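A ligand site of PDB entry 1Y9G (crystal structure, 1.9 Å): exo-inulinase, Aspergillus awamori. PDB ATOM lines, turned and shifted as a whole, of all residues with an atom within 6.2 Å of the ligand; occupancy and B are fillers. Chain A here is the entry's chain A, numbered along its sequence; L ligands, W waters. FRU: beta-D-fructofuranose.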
ATOM      1  N   ASN A  21      -5.809   9.523 -23.141  1.00  0.00           N
ATOM      2  CA  ASN A  21      -4.686  10.376 -23.552  1.00  0.00           C
ATOM      3  C   ASN A  21      -4.784  10.881 -25.024  1.00  0.00           C
ATOM      4  O   ASN A  21      -5.831  11.445 -25.401  1.00  0.00           O
ATOM      5  CB  ASN A  21      -3.262   9.852 -23.047  1.00  0.00           C
ATOM      6  CG  ASN A  21      -2.930   8.395 -23.465  1.00  0.00           C
ATOM      7  OD1 ASN A  21      -3.585   7.442 -23.033  1.00  0.00           O
ATOM      8  ND2 ASN A  21      -1.874   8.231 -24.311  1.00  0.00           N
ATOM      9  N   ASP A  22      -3.812  10.526 -25.853  1.00  0.00           N
ATOM     10  CA  ASP A  22      -3.529  11.271 -27.081  1.00  0.00           C
ATOM     11  C   ASP A  22      -4.697  11.261 -28.030  1.00  0.00           C
ATOM     12  O   ASP A  22      -5.387  10.222 -28.218  1.00  0.00           O
ATOM     13  CB  ASP A  22      -2.427  10.688 -27.902  1.00  0.00           C
ATOM     14  CG  ASP A  22      -1.180  10.323 -27.154  1.00  0.00           C
ATOM     15  OD1 ASP A  22      -0.974  10.597 -25.921  1.00  0.00           O
ATOM     16  OD2 ASP A  22      -0.292   9.768 -27.828  1.00  0.00           O
ATOM     17  N   GLN A  38      -6.673   7.707 -27.432  1.00  0.00           N
ATOM     18  CA  GLN A  38      -6.127   6.710 -26.540  1.00  0.00           C
ATOM     19  C   GLN A  38      -7.063   6.636 -25.369  1.00  0.00           C
ATOM     20  O   GLN A  38      -7.388   7.633 -24.728  1.00  0.00           O
ATOM     21  CB  GLN A  38      -4.706   7.076 -26.119  1.00  0.00           C
ATOM     22  CG  GLN A  38      -3.706   7.116 -27.228  1.00  0.00           C
ATOM     23  CD  GLN A  38      -3.376   5.693 -27.717  1.00  0.00           C
ATOM     24  OE1 GLN A  38      -4.048   5.188 -28.629  1.00  0.00           O
ATOM     25  NE2 GLN A  38      -2.424   5.056 -27.100  1.00  0.00           N
ATOM     26  N   TRP A  46      -4.150   5.005 -17.225  1.00  0.00           N
ATOM     27  CA  TRP A  46      -3.666   4.435 -18.474  1.00  0.00           C
ATOM     28  C   TRP A  46      -3.668   2.888 -18.361  1.00  0.00           C
ATOM     29  O   TRP A  46      -3.195   2.330 -17.368  1.00  0.00           O
ATOM     30  CB  TRP A  46      -2.279   4.948 -18.759  1.00  0.00           C
ATOM     31  CG  TRP A  46      -1.731   4.560 -20.144  1.00  0.00           C
ATOM     32  CD1 TRP A  46      -1.702   5.340 -21.264  1.00  0.00           C
ATOM     33  CD2 TRP A  46      -1.113   3.333 -20.506  1.00  0.00           C
ATOM     34  NE1 TRP A  46      -1.101   4.656 -22.303  1.00  0.00           N
ATOM     35  CE2 TRP A  46      -0.742   3.419 -21.862  1.00  0.00           C
ATOM     36  CE3 TRP A  46      -0.818   2.125 -19.797  1.00  0.00           C
ATOM     37  CZ2 TRP A  46      -0.097   2.347 -22.558  1.00  0.00           C
ATOM     38  CZ3 TRP A  46      -0.161   1.075 -20.479  1.00  0.00           C
ATOM     39  CH2 TRP A  46       0.168   1.210 -21.864  1.00  0.00           C
ATOM     40  N   ILE A  49      -5.125  -0.218 -23.588  1.00  0.00           N
ATOM     41  CA  ILE A  49      -5.222   0.890 -24.475  1.00  0.00           C
ATOM     42  C   ILE A  49      -5.905   0.565 -25.819  1.00  0.00           C
ATOM     43  O   ILE A  49      -5.517  -0.374 -26.554  1.00  0.00           O
ATOM     44  CB  ILE A  49      -3.864   1.593 -24.659  1.00  0.00           C
ATOM     45  CG1 ILE A  49      -3.453   2.342 -23.374  1.00  0.00           C
ATOM     46  CG2 ILE A  49      -3.923   2.499 -25.820  1.00  0.00           C
ATOM     47  CD1 ILE A  49      -4.379   3.501 -22.985  1.00  0.00           C
ATOM     48  N   TYR A  82      -3.749  -0.708 -28.857  1.00  0.00           N
ATOM     49  CA  TYR A  82      -3.779   0.148 -30.052  1.00  0.00           C
ATOM     50  C   TYR A  82      -3.253   1.464 -29.572  1.00  0.00           C
ATOM     51  O   TYR A  82      -4.001   2.319 -29.092  1.00  0.00           O
ATOM     52  CB  TYR A  82      -5.210   0.239 -30.659  1.00  0.00           C
ATOM     53  CG  TYR A  82      -5.679  -1.118 -31.134  1.00  0.00           C
ATOM     54  CD1 TYR A  82      -5.301  -1.595 -32.384  1.00  0.00           C
ATOM     55  CD2 TYR A  82      -6.501  -1.926 -30.339  1.00  0.00           C
ATOM     56  CE1 TYR A  82      -5.665  -2.910 -32.812  1.00  0.00           C
ATOM     57  CE2 TYR A  82      -6.855  -3.214 -30.745  1.00  0.00           C
ATOM     58  CZ  TYR A  82      -6.482  -3.684 -32.001  1.00  0.00           C
ATOM     59  OH  TYR A  82      -6.897  -4.955 -32.396  1.00  0.00           O
ATOM     60  N   PHE A  83      -1.936   1.615 -29.717  1.00  0.00           N
ATOM     61  CA  PHE A  83      -1.305   2.897 -29.445  1.00  0.00           C
ATOM     62  C   PHE A  83      -1.700   3.945 -30.513  1.00  0.00           C
ATOM     63  O   PHE A  83      -2.448   3.640 -31.449  1.00  0.00           O
ATOM     64  CB  PHE A  83       0.211   2.695 -29.279  1.00  0.00           C
ATOM     65  CG  PHE A  83       0.622   2.152 -27.887  1.00  0.00           C
ATOM     66  CD1 PHE A  83      -0.282   1.473 -27.097  1.00  0.00           C
ATOM     67  CD2 PHE A  83       1.941   2.313 -27.408  1.00  0.00           C
ATOM     68  CE1 PHE A  83       0.089   0.984 -25.822  1.00  0.00           C
ATOM     69  CE2 PHE A  83       2.303   1.805 -26.183  1.00  0.00           C
ATOM     70  CZ  PHE A  83       1.378   1.155 -25.393  1.00  0.00           C
ATOM     71  N   SER A  84      -1.041   5.113 -30.440  1.00  0.00           N
ATOM     72  CA  SER A  84      -1.452   6.269 -31.217  1.00  0.00           C
ATOM     73  C   SER A  84      -1.231   6.167 -32.744  1.00  0.00           C
ATOM     74  O   SER A  84      -0.439   5.398 -33.245  1.00  0.00           O
ATOM     75  CB  SER A  84      -0.850   7.578 -30.642  1.00  0.00           C
ATOM     76  OG  SER A  84      -1.473   7.917 -29.364  1.00  0.00           O
ATOM     77  N   GLY A  85      -2.008   6.942 -33.479  1.00  0.00           N
ATOM     78  CA  GLY A  85      -1.941   6.887 -34.917  1.00  0.00           C
ATOM     79  C   GLY A  85      -2.934   7.881 -35.506  1.00  0.00           C
ATOM     80  O   GLY A  85      -3.475   8.760 -34.807  1.00  0.00           O
ATOM     81  N   THR A 110       0.166   2.429 -34.026  1.00  0.00           N
ATOM     82  CA  THR A 110       1.132   1.549 -33.408  1.00  0.00           C
ATOM     83  C   THR A 110       0.492   0.390 -32.672  1.00  0.00           C
ATOM     84  O   THR A 110      -0.291   0.594 -31.772  1.00  0.00           O
ATOM     85  CB  THR A 110       1.970   2.382 -32.423  1.00  0.00           C
ATOM     86  OG1 THR A 110       2.697   3.367 -33.173  1.00  0.00           O
ATOM     87  CG2 THR A 110       3.012   1.453 -31.682  1.00  0.00           C
ATOM     88  N   GLN A 130       6.730  -2.614 -30.338  1.00  0.00           N
ATOM     89  CA  GLN A 130       5.883  -1.619 -31.060  1.00  0.00           C
ATOM     90  C   GLN A 130       6.167  -1.700 -32.573  1.00  0.00           C
ATOM     91  O   GLN A 130       7.328  -1.624 -33.049  1.00  0.00           O
ATOM     92  CB  GLN A 130       6.166  -0.208 -30.568  1.00  0.00           C
ATOM     93  CG  GLN A 130       5.794  -0.009 -29.067  1.00  0.00           C
ATOM     94  CD  GLN A 130       6.044   1.414 -28.507  1.00  0.00           C
ATOM     95  OE1 GLN A 130       6.717   2.210 -29.101  1.00  0.00           O
ATOM     96  NE2 GLN A 130       5.569   1.638 -27.277  1.00  0.00           N
ATOM     97  N   ARG A 169       6.886   4.373 -32.907  1.00  0.00           N
ATOM     98  CA  ARG A 169       5.477   4.607 -32.703  1.00  0.00           C
ATOM     99  C   ARG A 169       4.966   5.893 -33.334  1.00  0.00           C
ATOM    100  O   ARG A 169       5.720   6.746 -33.763  1.00  0.00           O
ATOM    101  CB  ARG A 169       5.110   4.453 -31.206  1.00  0.00           C
ATOM    102  CG  ARG A 169       5.758   5.439 -30.232  1.00  0.00           C
ATOM    103  CD  ARG A 169       5.222   5.304 -28.814  1.00  0.00           C
ATOM    104  NE  ARG A 169       5.955   6.109 -27.824  1.00  0.00           N
ATOM    105  CZ  ARG A 169       7.090   5.740 -27.259  1.00  0.00           C
ATOM    106  NH1 ARG A 169       7.667   4.584 -27.627  1.00  0.00           N
ATOM    107  NH2 ARG A 169       7.682   6.519 -26.373  1.00  0.00           N
ATOM    108  N   ASP A 170       3.622   5.958 -33.394  1.00  0.00           N
ATOM    109  CA  ASP A 170       2.814   7.205 -33.553  1.00  0.00           C
ATOM    110  C   ASP A 170       2.833   7.626 -35.003  1.00  0.00           C
ATOM    111  O   ASP A 170       3.251   8.748 -35.323  1.00  0.00           O
ATOM    112  CB  ASP A 170       3.321   8.361 -32.661  1.00  0.00           C
ATOM    113  CG  ASP A 170       3.191   8.088 -31.163  1.00  0.00           C
ATOM    114  OD1 ASP A 170       2.637   7.057 -30.704  1.00  0.00           O
ATOM    115  OD2 ASP A 170       3.696   8.849 -30.335  1.00  0.00           O
ATOM    116  N   TRP A 221      10.826  11.378 -28.082  1.00  0.00           N
ATOM    117  CA  TRP A 221      10.050  12.076 -29.131  1.00  0.00           C
ATOM    118  C   TRP A 221       8.776  11.276 -29.409  1.00  0.00           C
ATOM    119  O   TRP A 221       8.807  10.103 -29.624  1.00  0.00           O
ATOM    120  CB  TRP A 221      10.863  12.308 -30.397  1.00  0.00           C
ATOM    121  CG  TRP A 221      11.726  13.525 -30.316  1.00  0.00           C
ATOM    122  CD1 TRP A 221      12.231  14.155 -29.175  1.00  0.00           C
ATOM    123  CD2 TRP A 221      12.247  14.228 -31.397  1.00  0.00           C
ATOM    124  NE1 TRP A 221      12.990  15.234 -29.516  1.00  0.00           N
ATOM    125  CE2 TRP A 221      13.052  15.291 -30.893  1.00  0.00           C
ATOM    126  CE3 TRP A 221      12.107  14.114 -32.777  1.00  0.00           C
ATOM    127  CZ2 TRP A 221      13.630  16.231 -31.724  1.00  0.00           C
ATOM    128  CZ3 TRP A 221      12.759  15.028 -33.585  1.00  0.00           C
ATOM    129  CH2 TRP A 221      13.455  16.073 -33.060  1.00  0.00           C
ATOM    130  N   GLU A 222       7.645  11.955 -29.432  1.00  0.00           N
ATOM    131  CA  GLU A 222       6.364  11.297 -29.670  1.00  0.00           C
ATOM    132  C   GLU A 222       5.444  12.149 -30.574  1.00  0.00           C
ATOM    133  O   GLU A 222       5.738  13.342 -30.885  1.00  0.00           O
ATOM    134  CB  GLU A 222       5.694  10.939 -28.348  1.00  0.00           C
ATOM    135  CG  GLU A 222       6.531  10.135 -27.374  1.00  0.00           C
ATOM    136  CD  GLU A 222       5.809   9.815 -26.102  1.00  0.00           C
ATOM    137  OE1 GLU A 222       5.290  10.734 -25.399  1.00  0.00           O
ATOM    138  OE2 GLU A 222       5.754   8.611 -25.834  1.00  0.00           O
ATOM    139  N   CYS A 223       4.432  11.492 -31.133  1.00  0.00           N
ATOM    140  CA  CYS A 223       3.328  12.220 -31.798  1.00  0.00           C
ATOM    141  C   CYS A 223       3.786  13.197 -32.888  1.00  0.00           C
ATOM    142  O   CYS A 223       3.406  14.357 -32.873  1.00  0.00           O
ATOM    143  CB  CYS A 223       2.493  12.905 -30.734  1.00  0.00           C
ATOM    144  SG  CYS A 223       1.699  11.619 -29.627  1.00  0.00           S
ATOM    145  N   TYR A 294      -0.138  18.466 -25.008  1.00  0.00           N
ATOM    146  CA  TYR A 294       0.682  17.364 -25.459  1.00  0.00           C
ATOM    147  C   TYR A 294       0.017  16.469 -26.495  1.00  0.00           C
ATOM    148  O   TYR A 294      -1.170  16.499 -26.651  1.00  0.00           O
ATOM    149  CB  TYR A 294       1.107  16.538 -24.259  1.00  0.00           C
ATOM    150  CG  TYR A 294       2.238  15.586 -24.571  1.00  0.00           C
ATOM    151  CD1 TYR A 294       3.424  16.078 -25.038  1.00  0.00           C
ATOM    152  CD2 TYR A 294       2.116  14.185 -24.460  1.00  0.00           C
ATOM    153  CE1 TYR A 294       4.462  15.301 -25.364  1.00  0.00           C
ATOM    154  CE2 TYR A 294       3.230  13.351 -24.803  1.00  0.00           C
ATOM    155  CZ  TYR A 294       4.400  13.940 -25.252  1.00  0.00           C
ATOM    156  OH  TYR A 294       5.542  13.254 -25.658  1.00  0.00           O
ATOM    157  N   ALA A 295       0.834  15.674 -27.203  1.00  0.00           N
ATOM    158  CA  ALA A 295       0.335  14.696 -28.158  1.00  0.00           C
ATOM    159  C   ALA A 295      -0.486  15.406 -29.201  1.00  0.00           C
ATOM    160  O   ALA A 295      -1.492  14.882 -29.687  1.00  0.00           O
ATOM    161  CB  ALA A 295      -0.505  13.628 -27.456  1.00  0.00           C
ATOM    162  N   TRP A 312      -3.809  16.992 -26.312  1.00  0.00           N
ATOM    163  CA  TRP A 312      -4.218  16.419 -25.031  1.00  0.00           C
ATOM    164  C   TRP A 312      -3.939  17.438 -23.963  1.00  0.00           C
ATOM    165  O   TRP A 312      -2.852  17.877 -23.792  1.00  0.00           O
ATOM    166  CB  TRP A 312      -3.411  15.153 -24.764  1.00  0.00           C
ATOM    167  CG  TRP A 312      -3.729  14.421 -23.541  1.00  0.00           C
ATOM    168  CD1 TRP A 312      -4.959  14.096 -23.057  1.00  0.00           C
ATOM    169  CD2 TRP A 312      -2.771  13.824 -22.644  1.00  0.00           C
ATOM    170  NE1 TRP A 312      -4.817  13.330 -21.916  1.00  0.00           N
ATOM    171  CE2 TRP A 312      -3.474  13.157 -21.643  1.00  0.00           C
ATOM    172  CE3 TRP A 312      -1.391  13.850 -22.572  1.00  0.00           C
ATOM    173  CZ2 TRP A 312      -2.853  12.501 -20.586  1.00  0.00           C
ATOM    174  CZ3 TRP A 312      -0.761  13.182 -21.519  1.00  0.00           C
ATOM    175  CH2 TRP A 312      -1.498  12.522 -20.530  1.00  0.00           C
ATOM    176  N   TRP A 316       2.164  14.259 -18.560  1.00  0.00           N
ATOM    177  CA  TRP A 316       2.499  12.920 -17.988  1.00  0.00           C
ATOM    178  C   TRP A 316       3.122  12.960 -16.611  1.00  0.00           C
ATOM    179  O   TRP A 316       3.051  11.949 -15.936  1.00  0.00           O
ATOM    180  CB  TRP A 316       3.397  12.139 -18.915  1.00  0.00           C
ATOM    181  CG  TRP A 316       2.696  11.556 -20.110  1.00  0.00           C
ATOM    182  CD1 TRP A 316       2.877  11.884 -21.413  1.00  0.00           C
ATOM    183  CD2 TRP A 316       1.737  10.517 -20.086  1.00  0.00           C
ATOM    184  NE1 TRP A 316       2.054  11.124 -22.199  1.00  0.00           N
ATOM    185  CE2 TRP A 316       1.369  10.251 -21.401  1.00  0.00           C
ATOM    186  CE3 TRP A 316       1.157   9.773 -19.066  1.00  0.00           C
ATOM    187  CZ2 TRP A 316       0.434   9.300 -21.730  1.00  0.00           C
ATOM    188  CZ3 TRP A 316       0.237   8.799 -19.400  1.00  0.00           C
ATOM    189  CH2 TRP A 316      -0.093   8.566 -20.715  1.00  0.00           C
HETATM  190  C1  FRU L   1       2.192   9.841 -25.877  1.00  0.00           C
HETATM  191  C2  FRU L   1       1.936   8.354 -26.096  1.00  0.00           C
HETATM  192  C3  FRU L   1       2.310   7.863 -27.471  1.00  0.00           C
HETATM  193  C4  FRU L   1       1.787   6.407 -27.425  1.00  0.00           C
HETATM  194  C5  FRU L   1       0.589   6.493 -26.517  1.00  0.00           C
HETATM  195  C6  FRU L   1       0.321   5.312 -25.589  1.00  0.00           C
HETATM  196  O1  FRU L   1       1.295  10.389 -24.923  1.00  0.00           O
HETATM  197  O2  FRU L   1       2.963   7.721 -25.293  1.00  0.00           O
HETATM  198  O3  FRU L   1       3.675   8.061 -27.816  1.00  0.00           O
HETATM  199  O4  FRU L   1       1.321   6.017 -28.685  1.00  0.00           O
HETATM  200  O5  FRU L   1       0.793   7.653 -25.728  1.00  0.00           O
HETATM  201  O6  FRU L   1      -0.971   5.578 -25.025  1.00  0.00           O
HETATM  202  O   HOH W   1       3.861   5.419 -24.162  1.00  0.00           O
HETATM  203  O   HOH W   2       3.456   7.493 -22.059  1.00  0.00           O
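O1 of the ligand lies within hydrogen-bond range of OD1 of Asp 22 (2.5 Å).
O4 of the ligand lies within hydrogen-bond range of OD1 of Asp 170 (2.6 Å).
The side-chain carboxylate (OE2) of Glu 222 lies within hydrogen-bond range of an oxygen (O3) of the ligand (2.9 Å).
N of Ser 84 is in hydrogen-bond range of O4 of the ligand.
The side-chain amide nitrogen of Asn 21 is in hydrogen-bond range of an oxygen (O6) of the ligand.
The indole nitrogen of Trp 316 lies within hydrogen-bond range of an oxygen (O1) of the ligand (2.9 Å).
The side-chain amide nitrogen (NE2) of Gln 38 lies within hydrogen-bond range of an oxygen (O6) of the ligand (2.6 Å).
The indole nitrogen (NE1) of Trp 46 sits at hydrogen-bond distance from an oxygen (O6) of the ligand, at 2.9 Å.
O3 of the ligand is in hydrogen-bond range of NE of Arg 169, at 3.0 Å.
The side-chain hydroxyl (OG) of Ser 84 sits close to an oxygen (O4) of the ligand (3.4 Å).
Phe 83 touches the ligand.
CE2 of Tyr 294 touches O1 of the ligand, at 3.5 Å.
Hydrophobic or aromatic side chains within 4 Å of the ligand: Trp 46, Phe 83, Tyr 294 and Trp 316.
Within 4 Å of the ligand: Asn 21, Asp 22, Gln 38, Trp 46, Phe 83, Ser 84, Arg 169, Asp 170, Glu 222, Tyr 294 and Trp 316.
The nearest printed residue that does not touch the ligand is Cys 223 (4.2 Å).
The side-chain carboxylate (OD1) of Asp 22 sits at hydrogen-bond distance from the side-chain amide nitrogen (ND2) of Asn 21, 3.0 Å away.
The side-chain carboxylate of Asp 22 is in hydrogen-bond range of the side-chain sulfur of Cys 223 (3.3 Å).
The side-chain carboxylate of Glu 222 is in hydrogen-bond range of the side-chain hydroxyl of Tyr 294 (2.5 Å).
The backbone NH of Asn 21 is in hydrogen-bond range of the backbone carbonyl oxygen of Gln 38, 2.9 Å away.
The side-chain carboxylate of Glu 222 is in salt-bridge range of the guanidinium group of Arg 169, 2.9 Å away.
N of Cys 223 lies within hydrogen-bond range of OD2 of Asp 170 (2.9 Å).
The backbone NH of Trp 312 is in hydrogen-bond range of the backbone carbonyl oxygen of Tyr 294 (2.7 Å).
The guanidinium group of Arg 169 is in hydrogen-bond range of the side-chain amide oxygen of Gln 130, 3.0 Å away.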
